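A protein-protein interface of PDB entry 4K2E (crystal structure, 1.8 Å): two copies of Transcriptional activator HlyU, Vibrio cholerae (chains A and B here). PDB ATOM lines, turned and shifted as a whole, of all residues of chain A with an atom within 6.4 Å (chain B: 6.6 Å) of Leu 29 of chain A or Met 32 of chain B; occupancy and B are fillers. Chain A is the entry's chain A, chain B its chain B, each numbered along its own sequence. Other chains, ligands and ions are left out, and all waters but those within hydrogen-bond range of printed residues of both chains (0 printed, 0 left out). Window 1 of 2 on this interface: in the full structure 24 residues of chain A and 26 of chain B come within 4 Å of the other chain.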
ATOM      1  N   SER A  22       9.481 -16.113  -4.388  1.00  0.00           N
ATOM      2  CA  SER A  22       8.356 -16.559  -5.191  1.00  0.00           C
ATOM      3  C   SER A  22       7.572 -17.615  -4.433  1.00  0.00           C
ATOM      4  O   SER A  22       6.368 -17.552  -4.422  1.00  0.00           O
ATOM      5  CB  SER A  22       8.749 -17.046  -6.596  1.00  0.00           C
ATOM      6  OG  SER A  22       9.543 -18.220  -6.564  1.00  0.00           O
ATOM      7  N   LYS A  24       7.003 -17.981  -1.078  1.00  0.00           N
ATOM      8  CA  LYS A  24       6.154 -17.394  -0.035  1.00  0.00           C
ATOM      9  C   LYS A  24       4.991 -16.588  -0.628  1.00  0.00           C
ATOM     10  O   LYS A  24       3.801 -16.683  -0.196  1.00  0.00           O
ATOM     11  CB  LYS A  24       6.982 -16.491   0.879  1.00  0.00           C
ATOM     12  CG  LYS A  24       6.160 -15.764   1.949  1.00  0.00           C
ATOM     13  CD  LYS A  24       7.065 -15.060   2.969  1.00  0.00           C
ATOM     14  CE  LYS A  24       6.247 -14.342   4.050  1.00  0.00           C
ATOM     15  NZ  LYS A  24       7.060 -13.334   4.812  1.00  0.00           N
ATOM     16  N   ALA A  25       5.343 -15.791  -1.635  1.00  0.00           N
ATOM     17  CA  ALA A  25       4.315 -15.049  -2.349  1.00  0.00           C
ATOM     18  C   ALA A  25       3.279 -16.020  -2.890  1.00  0.00           C
ATOM     19  O   ALA A  25       2.088 -15.742  -2.864  1.00  0.00           O
ATOM     20  CB  ALA A  25       4.925 -14.260  -3.466  1.00  0.00           C
ATOM     21  N   VAL A  26       3.739 -17.177  -3.354  1.00  0.00           N
ATOM     22  CA  VAL A  26       2.852 -18.127  -4.000  1.00  0.00           C
ATOM     23  C   VAL A  26       1.914 -18.785  -2.970  1.00  0.00           C
ATOM     24  O   VAL A  26       0.765 -19.069  -3.278  1.00  0.00           O
ATOM     25  CB  VAL A  26       3.629 -19.173  -4.826  1.00  0.00           C
ATOM     26  CG1 VAL A  26       2.758 -20.339  -5.193  1.00  0.00           C
ATOM     27  CG2 VAL A  26       4.179 -18.526  -6.123  1.00  0.00           C
ATOM     28  N   VAL A  27       2.390 -18.997  -1.745  1.00  0.00           N
ATOM     29  CA  VAL A  27       1.471 -19.450  -0.684  1.00  0.00           C
ATOM     30  C   VAL A  27       0.312 -18.478  -0.561  1.00  0.00           C
ATOM     31  O   VAL A  27      -0.885 -18.870  -0.541  1.00  0.00           O
ATOM     32  CB  VAL A  27       2.139 -19.548   0.696  1.00  0.00           C
ATOM     33  CG1 VAL A  27       1.054 -19.848   1.775  1.00  0.00           C
ATOM     34  CG2 VAL A  27       3.210 -20.606   0.663  1.00  0.00           C
ATOM     35  N   LEU A  28       0.664 -17.201  -0.496  1.00  0.00           N
ATOM     36  CA  LEU A  28      -0.386 -16.198  -0.423  1.00  0.00           C
ATOM     37  C   LEU A  28      -1.332 -16.199  -1.635  1.00  0.00           C
ATOM     38  O   LEU A  28      -2.551 -16.143  -1.499  1.00  0.00           O
ATOM     39  CB  LEU A  28       0.238 -14.829  -0.270  1.00  0.00           C
ATOM     40  CG  LEU A  28      -0.776 -13.698  -0.327  1.00  0.00           C
ATOM     41  CD1 LEU A  28      -1.434 -13.520   1.047  1.00  0.00           C
ATOM     42  CD2 LEU A  28      -0.072 -12.426  -0.800  1.00  0.00           C
ATOM     43  N   LEU A  29      -0.749 -16.265  -2.835  1.00  0.00           N
ATOM     44  CA  LEU A  29      -1.532 -16.234  -4.068  1.00  0.00           C
ATOM     45  C   LEU A  29      -2.458 -17.450  -4.191  1.00  0.00           C
ATOM     46  O   LEU A  29      -3.592 -17.324  -4.657  1.00  0.00           O
ATOM     47  CB  LEU A  29      -0.586 -16.119  -5.308  1.00  0.00           C
ATOM     48  CG  LEU A  29       0.189 -14.798  -5.300  1.00  0.00           C
ATOM     49  CD1 LEU A  29       1.414 -14.846  -6.192  1.00  0.00           C
ATOM     50  CD2 LEU A  29      -0.740 -13.704  -5.769  1.00  0.00           C
ATOM     51  N   LYS A  30      -1.959 -18.621  -3.809  1.00  0.00           N
ATOM     52  CA  LYS A  30      -2.733 -19.849  -3.888  1.00  0.00           C
ATOM     53  C   LYS A  30      -3.910 -19.762  -2.887  1.00  0.00           C
ATOM     54  O   LYS A  30      -5.009 -20.214  -3.203  1.00  0.00           O
ATOM     55  CB  LYS A  30      -1.876 -21.083  -3.554  1.00  0.00           C
ATOM     56  CG  LYS A  30      -0.902 -21.479  -4.671  1.00  0.00           C
ATOM     57  CD  LYS A  30      -0.214 -22.811  -4.405  1.00  0.00           C
ATOM     58  CE  LYS A  30       0.595 -23.246  -5.608  1.00  0.00           C
ATOM     59  NZ  LYS A  30       1.618 -24.277  -5.256  1.00  0.00           N
ATOM     60  N   ALA A  31      -3.683 -19.138  -1.739  1.00  0.00           N
ATOM     61  CA  ALA A  31      -4.800 -18.995  -0.793  1.00  0.00           C
ATOM     62  C   ALA A  31      -5.856 -18.015  -1.353  1.00  0.00           C
ATOM     63  O   ALA A  31      -7.061 -18.258  -1.227  1.00  0.00           O
ATOM     64  CB  ALA A  31      -4.321 -18.615   0.609  1.00  0.00           C
ATOM     65  N   MET A  32      -5.408 -16.961  -2.039  1.00  0.00           N
ATOM     66  CA  MET A  32      -6.336 -16.032  -2.689  1.00  0.00           C
ATOM     67  C   MET A  32      -7.019 -16.461  -3.976  1.00  0.00           C
ATOM     68  O   MET A  32      -8.010 -15.848  -4.394  1.00  0.00           O
ATOM     69  CB  MET A  32      -5.629 -14.682  -2.944  1.00  0.00           C
ATOM     70  CG  MET A  32      -5.070 -14.125  -1.626  1.00  0.00           C
ATOM     71  SD  MET A  32      -4.241 -12.545  -2.012  1.00  0.00           S
ATOM     72  CE  MET A  32      -5.603 -11.740  -2.814  1.00  0.00           C
ATOM     73  N   ALA A  33      -6.449 -17.457  -4.649  1.00  0.00           N
ATOM     74  CA  ALA A  33      -6.841 -17.782  -6.002  1.00  0.00           C
ATOM     75  C   ALA A  33      -8.023 -18.740  -6.002  1.00  0.00           C
ATOM     76  O   ALA A  33      -7.936 -19.839  -6.528  1.00  0.00           O
ATOM     77  CB  ALA A  33      -5.670 -18.408  -6.746  1.00  0.00           C
ATOM     78  N   ASN A  34      -9.134 -18.302  -5.429  1.00  0.00           N
ATOM     79  CA  ASN A  34     -10.329 -19.131  -5.339  1.00  0.00           C
ATOM     80  C   ASN A  34     -11.466 -18.152  -5.103  1.00  0.00           C
ATOM     81  O   ASN A  34     -11.334 -17.292  -4.252  1.00  0.00           O
ATOM     82  CB  ASN A  34     -10.207 -20.086  -4.157  1.00  0.00           C
ATOM     83  CG  ASN A  34     -11.500 -20.799  -3.868  1.00  0.00           C
ATOM     84  OD1 ASN A  34     -12.332 -20.296  -3.131  1.00  0.00           O
ATOM     85  ND2 ASN A  34     -11.693 -21.954  -4.486  1.00  0.00           N
ATOM     86  N   ARG A  37     -12.728 -17.948  -1.366  1.00  0.00           N
ATOM     87  CA  ARG A  37     -11.746 -17.418  -0.415  1.00  0.00           C
ATOM     88  C   ARG A  37     -11.453 -15.939  -0.666  1.00  0.00           C
ATOM     89  O   ARG A  37     -11.371 -15.155   0.289  1.00  0.00           O
ATOM     90  CB  ARG A  37     -10.446 -18.239  -0.381  1.00  0.00           C
ATOM     91  CG  ARG A  37     -10.612 -19.612   0.224  1.00  0.00           C
ATOM     92  CD  ARG A  37      -9.307 -20.397   0.394  1.00  0.00           C
ATOM     93  NE  ARG A  37      -8.444 -20.516  -0.805  1.00  0.00           N
ATOM     94  CZ  ARG A  37      -8.419 -21.541  -1.659  1.00  0.00           C
ATOM     95  NH1 ARG A  37      -9.262 -22.568  -1.538  1.00  0.00           N
ATOM     96  NH2 ARG A  37      -7.545 -21.531  -2.673  1.00  0.00           N
ATOM     97  N   MET A  99      -2.588  -6.521  -0.493  1.00  0.00           N
ATOM     98  CA  MET A  99      -3.067  -7.125  -1.726  1.00  0.00           C
ATOM     99  C   MET A  99      -4.580  -6.935  -1.889  1.00  0.00           C
ATOM    100  O   MET A  99      -5.044  -6.623  -2.976  1.00  0.00           O
ATOM    101  CB  MET A  99      -2.663  -8.603  -1.810  1.00  0.00           C
ATOM    102  CG  MET A  99      -3.126  -9.301  -3.097  1.00  0.00           C
ATOM    103  SD  MET A  99      -2.400  -8.615  -4.620  1.00  0.00           S
ATOM    104  CE  MET A  99      -0.645  -8.583  -4.204  1.00  0.00           C
ATOM    105  N   VAL B  27      -9.162 -15.198 -12.074  1.00  0.00           N
ATOM    106  CA  VAL B  27      -8.359 -15.642 -13.237  1.00  0.00           C
ATOM    107  C   VAL B  27      -6.915 -15.129 -13.155  1.00  0.00           C
ATOM    108  O   VAL B  27      -5.947 -15.902 -13.324  1.00  0.00           O
ATOM    109  CB  VAL B  27      -8.997 -15.236 -14.581  1.00  0.00           C
ATOM    110  CG1 VAL B  27      -7.986 -15.421 -15.744  1.00  0.00           C
ATOM    111  CG2 VAL B  27     -10.250 -16.040 -14.827  1.00  0.00           C
ATOM    112  N   LEU B  28      -6.754 -13.844 -12.865  1.00  0.00           N
ATOM    113  CA  LEU B  28      -5.395 -13.327 -12.679  1.00  0.00           C
ATOM    114  C   LEU B  28      -4.612 -14.049 -11.563  1.00  0.00           C
ATOM    115  O   LEU B  28      -3.449 -14.446 -11.739  1.00  0.00           O
ATOM    116  CB  LEU B  28      -5.401 -11.830 -12.367  1.00  0.00           C
ATOM    117  CG  LEU B  28      -5.927 -10.940 -13.508  1.00  0.00           C
ATOM    118  CD1 LEU B  28      -5.431  -9.519 -13.303  1.00  0.00           C
ATOM    119  CD2 LEU B  28      -5.532 -11.454 -14.928  1.00  0.00           C
ATOM    120  N   LEU B  29      -5.240 -14.195 -10.410  1.00  0.00           N
ATOM    121  CA  LEU B  29      -4.555 -14.773  -9.260  1.00  0.00           C
ATOM    122  C   LEU B  29      -4.163 -16.215  -9.534  1.00  0.00           C
ATOM    123  O   LEU B  29      -3.101 -16.631  -9.130  1.00  0.00           O
ATOM    124  CB  LEU B  29      -5.433 -14.691  -8.011  1.00  0.00           C
ATOM    125  CG  LEU B  29      -5.697 -13.265  -7.550  1.00  0.00           C
ATOM    126  CD1 LEU B  29      -6.938 -13.197  -6.640  1.00  0.00           C
ATOM    127  CD2 LEU B  29      -4.472 -12.760  -6.794  1.00  0.00           C
ATOM    128  N   LYS B  30      -5.026 -16.970 -10.217  1.00  0.00           N
ATOM    129  CA  LYS B  30      -4.729 -18.346 -10.586  1.00  0.00           C
ATOM    130  C   LYS B  30      -3.536 -18.363 -11.531  1.00  0.00           C
ATOM    131  O   LYS B  30      -2.674 -19.244 -11.421  1.00  0.00           O
ATOM    132  CB  LYS B  30      -5.932 -19.042 -11.244  1.00  0.00           C
ATOM    133  CG  LYS B  30      -6.967 -19.537 -10.225  1.00  0.00           C
ATOM    134  CD  LYS B  30      -8.110 -20.310 -10.869  1.00  0.00           C
ATOM    135  CE  LYS B  30      -9.020 -20.923  -9.801  1.00  0.00           C
ATOM    136  NZ  LYS B  30     -10.203 -21.539 -10.454  1.00  0.00           N
ATOM    137  N   ALA B  31      -3.456 -17.371 -12.415  1.00  0.00           N
ATOM    138  CA  ALA B  31      -2.306 -17.337 -13.336  1.00  0.00           C
ATOM    139  C   ALA B  31      -1.034 -17.010 -12.543  1.00  0.00           C
ATOM    140  O   ALA B  31       0.039 -17.532 -12.831  1.00  0.00           O
ATOM    141  CB  ALA B  31      -2.530 -16.334 -14.473  1.00  0.00           C
ATOM    142  N   MET B  32      -1.160 -16.204 -11.493  1.00  0.00           N
ATOM    143  CA  MET B  32       0.029 -15.816 -10.743  1.00  0.00           C
ATOM    144  C   MET B  32       0.455 -16.841  -9.727  1.00  0.00           C
ATOM    145  O   MET B  32       1.582 -16.758  -9.219  1.00  0.00           O
ATOM    146  CB  MET B  32      -0.166 -14.444 -10.065  1.00  0.00           C
ATOM    147  CG  MET B  32      -0.615 -13.342 -11.039  1.00  0.00           C
ATOM    148  SD  MET B  32      -0.814 -11.804 -10.146  1.00  0.00           S
ATOM    149  CE  MET B  32       0.827 -11.688  -9.536  1.00  0.00           C
ATOM    150  N   ALA B  33      -0.456 -17.757  -9.366  1.00  0.00           N
ATOM    151  CA  ALA B  33      -0.249 -18.606  -8.198  1.00  0.00           C
ATOM    152  C   ALA B  33       0.593 -19.820  -8.563  1.00  0.00           C
ATOM    153  O   ALA B  33       0.208 -20.954  -8.315  1.00  0.00           O
ATOM    154  CB  ALA B  33      -1.590 -19.054  -7.579  1.00  0.00           C
ATOM    155  N   ASN B  34       1.753 -19.581  -9.142  1.00  0.00           N
ATOM    156  CA  ASN B  34       2.630 -20.682  -9.544  1.00  0.00           C
ATOM    157  C   ASN B  34       4.043 -20.109  -9.538  1.00  0.00           C
ATOM    158  O   ASN B  34       4.242 -19.032 -10.056  1.00  0.00           O
ATOM    159  CB  ASN B  34       2.240 -21.184 -10.943  1.00  0.00           C
ATOM    160  CG  ASN B  34       3.287 -22.147 -11.540  1.00  0.00           C
ATOM    161  OD1 ASN B  34       4.308 -21.719 -12.067  1.00  0.00           O
ATOM    162  ND2 ASN B  34       3.033 -23.438 -11.431  1.00  0.00           N
ATOM    163  N   GLU B  35       5.025 -20.795  -8.967  1.00  0.00           N
ATOM    164  CA  GLU B  35       6.320 -20.122  -8.785  1.00  0.00           C
ATOM    165  C   GLU B  35       6.962 -19.702 -10.108  1.00  0.00           C
ATOM    166  O   GLU B  35       7.467 -18.588 -10.222  1.00  0.00           O
ATOM    167  CB  GLU B  35       7.299 -20.966  -7.979  1.00  0.00           C
ATOM    168  CG  GLU B  35       6.957 -21.091  -6.504  1.00  0.00           C
ATOM    169  CD  GLU B  35       7.718 -22.226  -5.878  1.00  0.00           C
ATOM    170  OE1 GLU B  35       8.659 -22.724  -6.537  1.00  0.00           O
ATOM    171  OE2 GLU B  35       7.355 -22.648  -4.760  1.00  0.00           O
ATOM    172  N   ARG B  37       5.448 -19.218 -13.158  1.00  0.00           N
ATOM    173  CA  ARG B  37       4.670 -18.138 -13.775  1.00  0.00           C
ATOM    174  C   ARG B  37       4.908 -16.784 -13.101  1.00  0.00           C
ATOM    175  O   ARG B  37       5.060 -15.742 -13.794  1.00  0.00           O
ATOM    176  CB  ARG B  37       3.169 -18.464 -13.867  1.00  0.00           C
ATOM    177  CG  ARG B  37       2.886 -19.626 -14.837  1.00  0.00           C
ATOM    178  CD  ARG B  37       1.375 -19.783 -15.165  1.00  0.00           C
ATOM    179  NE  ARG B  37       0.466 -19.965 -14.027  1.00  0.00           N
ATOM    180  CZ  ARG B  37       0.070 -21.139 -13.526  1.00  0.00           C
ATOM    181  NH1 ARG B  37       0.528 -22.290 -14.014  1.00  0.00           N
ATOM    182  NH2 ARG B  37      -0.782 -21.174 -12.509  1.00  0.00           N
ATOM    183  N   LEU B  38       4.965 -16.785 -11.769  1.00  0.00           N
ATOM    184  CA  LEU B  38       5.188 -15.538 -11.049  1.00  0.00           C
ATOM    185  C   LEU B  38       6.584 -14.997 -11.367  1.00  0.00           C
ATOM    186  O   LEU B  38       6.757 -13.796 -11.573  1.00  0.00           O
ATOM    187  CB  LEU B  38       5.064 -15.738  -9.548  1.00  0.00           C
ATOM    188  CG  LEU B  38       5.243 -14.489  -8.694  1.00  0.00           C
ATOM    189  CD1 LEU B  38       4.247 -13.429  -9.181  1.00  0.00           C
ATOM    190  CD2 LEU B  38       4.992 -14.835  -7.225  1.00  0.00           C
ATOM    191  N   GLN B  39       7.576 -15.882 -11.393  1.00  0.00           N
ATOM    192  CA  GLN B  39       8.945 -15.469 -11.737  1.00  0.00           C
ATOM    193  C   GLN B  39       9.002 -14.764 -13.093  1.00  0.00           C
ATOM    194  O   GLN B  39       9.660 -13.704 -13.245  1.00  0.00           O
ATOM    195  CB  GLN B  39       9.866 -16.688 -11.747  1.00  0.00           C
ATOM    196  CG  GLN B  39      10.174 -17.189 -10.366  1.00  0.00           C
ATOM    197  CD  GLN B  39      10.880 -18.527 -10.358  1.00  0.00           C
ATOM    198  OE1 GLN B  39      11.434 -18.963 -11.370  1.00  0.00           O
ATOM    199  NE2 GLN B  39      10.850 -19.193  -9.210  1.00  0.00           N
ATOM    200  N   LEU B  41       6.536 -13.271 -14.685  1.00  0.00           N
ATOM    201  CA  LEU B  41       5.896 -11.968 -14.566  1.00  0.00           C
ATOM    202  C   LEU B  41       6.761 -10.916 -13.856  1.00  0.00           C
ATOM    203  O   LEU B  41       6.768  -9.735 -14.254  1.00  0.00           O
ATOM    204  CB  LEU B  41       4.542 -12.109 -13.852  1.00  0.00           C
ATOM    205  CG  LEU B  41       3.469 -12.945 -14.565  1.00  0.00           C
ATOM    206  CD1 LEU B  41       2.300 -13.267 -13.620  1.00  0.00           C
ATOM    207  CD2 LEU B  41       2.974 -12.240 -15.842  1.00  0.00           C
ATOM    208  N   TRP B  71      -0.070 -20.282 -20.876  1.00  0.00           N
ATOM    209  CA  TRP B  71      -1.045 -19.938 -19.813  1.00  0.00           C
ATOM    210  C   TRP B  71      -1.142 -18.415 -19.627  1.00  0.00           C
ATOM    211  O   TRP B  71      -2.240 -17.865 -19.650  1.00  0.00           O
ATOM    212  CB  TRP B  71      -0.706 -20.696 -18.522  1.00  0.00           C
ATOM    213  CG  TRP B  71      -1.701 -20.586 -17.349  1.00  0.00           C
ATOM    214  CD1 TRP B  71      -2.345 -19.459 -16.898  1.00  0.00           C
ATOM    215  CD2 TRP B  71      -2.098 -21.645 -16.479  1.00  0.00           C
ATOM    216  NE1 TRP B  71      -3.119 -19.765 -15.793  1.00  0.00           N
ATOM    217  CE2 TRP B  71      -2.995 -21.103 -15.522  1.00  0.00           C
ATOM    218  CE3 TRP B  71      -1.789 -23.008 -16.411  1.00  0.00           C
ATOM    219  CZ2 TRP B  71      -3.590 -21.874 -14.526  1.00  0.00           C
ATOM    220  CZ3 TRP B  71      -2.387 -23.777 -15.412  1.00  0.00           C
ATOM    221  CH2 TRP B  71      -3.275 -23.203 -14.489  1.00  0.00           C
ATOM    222  N   LEU B  72       0.005 -17.742 -19.502  1.00  0.00           N
ATOM    223  CA  LEU B  72       0.017 -16.280 -19.351  1.00  0.00           C
ATOM    224  C   LEU B  72      -0.606 -15.539 -20.542  1.00  0.00           C
ATOM    225  O   LEU B  72      -1.275 -14.525 -20.360  1.00  0.00           O
ATOM    226  CB  LEU B  72       1.448 -15.757 -19.085  1.00  0.00           C
ATOM    227  CG  LEU B  72       2.053 -16.261 -17.765  1.00  0.00           C
ATOM    228  CD1 LEU B  72       3.496 -15.765 -17.672  1.00  0.00           C
ATOM    229  CD2 LEU B  72       1.134 -15.864 -16.481  1.00  0.00           C
ATOM    230  N   LEU B  77      -2.270 -11.942 -19.332  1.00  0.00           N
ATOM    231  CA  LEU B  77      -1.317 -11.290 -18.445  1.00  0.00           C
ATOM    232  C   LEU B  77      -0.082 -10.778 -19.184  1.00  0.00           C
ATOM    233  O   LEU B  77       0.714 -10.036 -18.615  1.00  0.00           O
ATOM    234  CB  LEU B  77      -0.826 -12.234 -17.376  1.00  0.00           C
ATOM    235  CG  LEU B  77      -1.885 -12.544 -16.314  1.00  0.00           C
ATOM    236  CD1 LEU B  77      -2.784 -13.664 -16.762  1.00  0.00           C
ATOM    237  CD2 LEU B  77      -1.207 -12.844 -15.002  1.00  0.00           C
ATOM    238  N   GLU B  95      -3.897  -3.897 -14.374  1.00  0.00           N
ATOM    239  CA  GLU B  95      -4.125  -4.713 -13.192  1.00  0.00           C
ATOM    240  C   GLU B  95      -2.931  -5.591 -12.922  1.00  0.00           C
ATOM    241  O   GLU B  95      -2.441  -5.681 -11.802  1.00  0.00           O
ATOM    242  CB  GLU B  95      -5.401  -5.571 -13.344  1.00  0.00           C
ATOM    243  CG  GLU B  95      -6.723  -4.767 -13.405  1.00  0.00           C
ATOM    244  CD  GLU B  95      -7.069  -4.266 -14.807  1.00  0.00           C
ATOM    245  OE1 GLU B  95      -6.530  -4.815 -15.794  1.00  0.00           O
ATOM    246  OE2 GLU B  95      -7.880  -3.313 -14.919  1.00  0.00           O
ATOM    247  N   VAL B  96      -2.441  -6.244 -13.964  1.00  0.00           N
ATOM    248  CA  VAL B  96      -1.349  -7.168 -13.794  1.00  0.00           C
ATOM    249  C   VAL B  96      -0.093  -6.421 -13.350  1.00  0.00           C
ATOM    250  O   VAL B  96       0.646  -6.880 -12.461  1.00  0.00           O
ATOM    251  CB  VAL B  96      -1.076  -7.887 -15.127  1.00  0.00           C
ATOM    252  CG1 VAL B  96       0.253  -8.563 -15.095  1.00  0.00           C
ATOM    253  CG2 VAL B  96      -2.209  -8.872 -15.430  1.00  0.00           C
ATOM    254  N   MET B  99      -0.371  -5.319  -9.762  1.00  0.00           N
ATOM    255  CA  MET B  99      -0.229  -6.490  -8.886  1.00  0.00           C
ATOM    256  C   MET B  99       1.236  -6.933  -8.753  1.00  0.00           C
ATOM    257  O   MET B  99       1.697  -7.187  -7.636  1.00  0.00           O
ATOM    258  CB  MET B  99      -1.170  -7.657  -9.291  1.00  0.00           C
ATOM    259  CG  MET B  99      -2.663  -7.357  -9.178  1.00  0.00           C
ATOM    260  SD  MET B  99      -3.745  -8.522 -10.078  1.00  0.00           S
ATOM    261  CE  MET B  99      -3.658  -9.982  -9.038  1.00  0.00           C
ATOM    262  N   ILE B 100       1.969  -6.990  -9.876  1.00  0.00           N
ATOM    263  CA  ILE B 100       3.373  -7.374  -9.871  1.00  0.00           C
ATOM    264  C   ILE B 100       4.190  -6.345  -9.139  1.00  0.00           C
ATOM    265  O   ILE B 100       5.081  -6.710  -8.393  1.00  0.00           O
ATOM    266  CB  ILE B 100       3.980  -7.583 -11.308  1.00  0.00           C
ATOM    267  CG1 ILE B 100       3.268  -8.712 -12.035  1.00  0.00           C
ATOM    268  CG2 ILE B 100       5.488  -7.878 -11.249  1.00  0.00           C
ATOM    269  CD1 ILE B 100       3.108  -9.939 -11.204  1.00  0.00           C
ATOM    270  N   LEU B 103       3.614  -6.911  -5.459  1.00  0.00           N
ATOM    271  CA  LEU B 103       4.296  -8.126  -5.003  1.00  0.00           C
ATOM    272  C   LEU B 103       5.794  -7.971  -4.894  1.00  0.00           C
ATOM    273  O   LEU B 103       6.429  -8.499  -3.973  1.00  0.00           O
ATOM    274  CB  LEU B 103       3.956  -9.313  -5.905  1.00  0.00           C
ATOM    275  CG  LEU B 103       2.528  -9.819  -5.685  1.00  0.00           C
ATOM    276  CD1 LEU B 103       2.236 -10.800  -6.749  1.00  0.00           C
ATOM    277  CD2 LEU B 103       2.403 -10.516  -4.337  1.00  0.00           C
ATOM    278  N   TYR B 107       7.647  -8.644  -1.369  1.00  0.00           N
ATOM    279  CA  TYR B 107       8.455  -9.862  -1.248  1.00  0.00           C
ATOM    280  C   TYR B 107       9.904  -9.720  -1.729  1.00  0.00           C
ATOM    281  O   TYR B 107      10.755 -10.551  -1.399  1.00  0.00           O
ATOM    282  CB  TYR B 107       7.755 -11.050  -1.935  1.00  0.00           C
ATOM    283  CG  TYR B 107       6.467 -11.437  -1.232  1.00  0.00           C
ATOM    284  CD1 TYR B 107       6.495 -12.227  -0.092  1.00  0.00           C
ATOM    285  CD2 TYR B 107       5.240 -10.979  -1.684  1.00  0.00           C
ATOM    286  CE1 TYR B 107       5.333 -12.569   0.571  1.00  0.00           C
ATOM    287  CE2 TYR B 107       4.061 -11.305  -1.020  1.00  0.00           C
ATOM    288  CZ  TYR B 107       4.119 -12.110   0.105  1.00  0.00           C
ATOM    289  OH  TYR B 107       2.962 -12.457   0.784  1.00  0.00           O
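Ser 22 of chain A touches Glu 35 of chain B.
CG of Lys 24 of chain A touches CE1 of Tyr 107 of chain B, at 3.6 Å.
Ala 25 of chain A touches Tyr 107 of chain B.
Asn 34 of chain B touches Val 26 of chain A.
O of Met 32 of chain B touches CD1 of Leu 29 of chain A, 3.6 Å away.
Leu 29 of chain A touches Ala 33 of chain B.
Leu 29 of chain A touches Leu 38 of chain B.
Met 32 of chain A touches Leu 29 of chain B (O to CD1, 3.6 Å).
Ala 33 of chain A touches Leu 29 of chain B.
O of Ala 33 of chain A touches CE of Lys 30 of chain B, at 3.6 Å.
The guanidinium group of Arg 37 of chain A sits at hydrogen-bond distance from the backbone carbonyl oxygen of Lys 30 of chain A, at 2.9 Å.
The backbone carbonyl oxygen (O) of Lys 30 of chain B sits at hydrogen-bond distance from the guanidinium group (NH2) of Arg 37 of chain B (2.9 Å).
OD1 of Asn 34 of chain B is in hydrogen-bond range of N of Arg 37 of chain B (3.0 Å).
The side-chain amide nitrogen of Gln 39 of chain B lies within hydrogen-bond range of the side-chain hydroxyl of Ser 22 of chain A.
Leu 29 of chain B touches its own counterpart, Leu 29 of chain A.
Leu 29 of chain A touches Met 32 of chain B, and with the chains exchanged Met 32 of chain A touches Leu 29 of chain B.
Leu 29 of chain A touches Ala 33 of chain B, and with the chains exchanged Ala 33 of chain A touches Leu 29 of chain B.
Lys 30 of chain A touches Ala 33 of chain B, and with the chains exchanged Ala 33 of chain A touches Lys 30 of chain B.
Positions printed for both chains: 27, 28, 29, 30, 31, 32, 33, 34, 37 and 99.
Hydrophobic or aromatic side chains of chain A that line the printed part of chain B: Ala 25, Val 26, Leu 28, Leu 29, Ala 33 and Met 99.
Among the printed residues, no Asp or Glu carboxylate lies within 4 Å of a Lys or Arg side-chain nitrogen of the other chain.
Printed residues of chain B within 4 Å of Ser 22 of chain A: Glu 35 (3.8 Å) and Gln 39 (3.1 Å).
Printed residues of chain B within 4 Å of Lys 24 of chain A: Tyr 107 (3.6 Å).
Of the printed residues of chain B, Leu 29 of chain A touches Leu 29 (3.98 Å), Met 32 (3.6 Å), Ala 33 (3.8 Å) and Leu 38 (3.7 Å).
Arg 37 of chain A touches none of the printed residues of chain B.
Of chain A, only Leu 29 comes within 4 Å of Met 32 of chain B.
Of the printed residues of chain A, Asn 34 of chain B touches Val 26.
Leu 77 of chain B touches none of the printed residues of chain A.
Of the printed residues of chain A, Tyr 107 of chain B touches Lys 24 (3.6 Å), Ala 25 (3.7 Å) and Leu 28 (3.4 Å).
The nearest printed residue of chain B that does not touch Leu 29 of chain A is Leu 103 of chain B (4.2 Å).
The nearest residue of chain A that does not touch Met 32 of chain B is Val 26 of chain A (4.4 Å).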
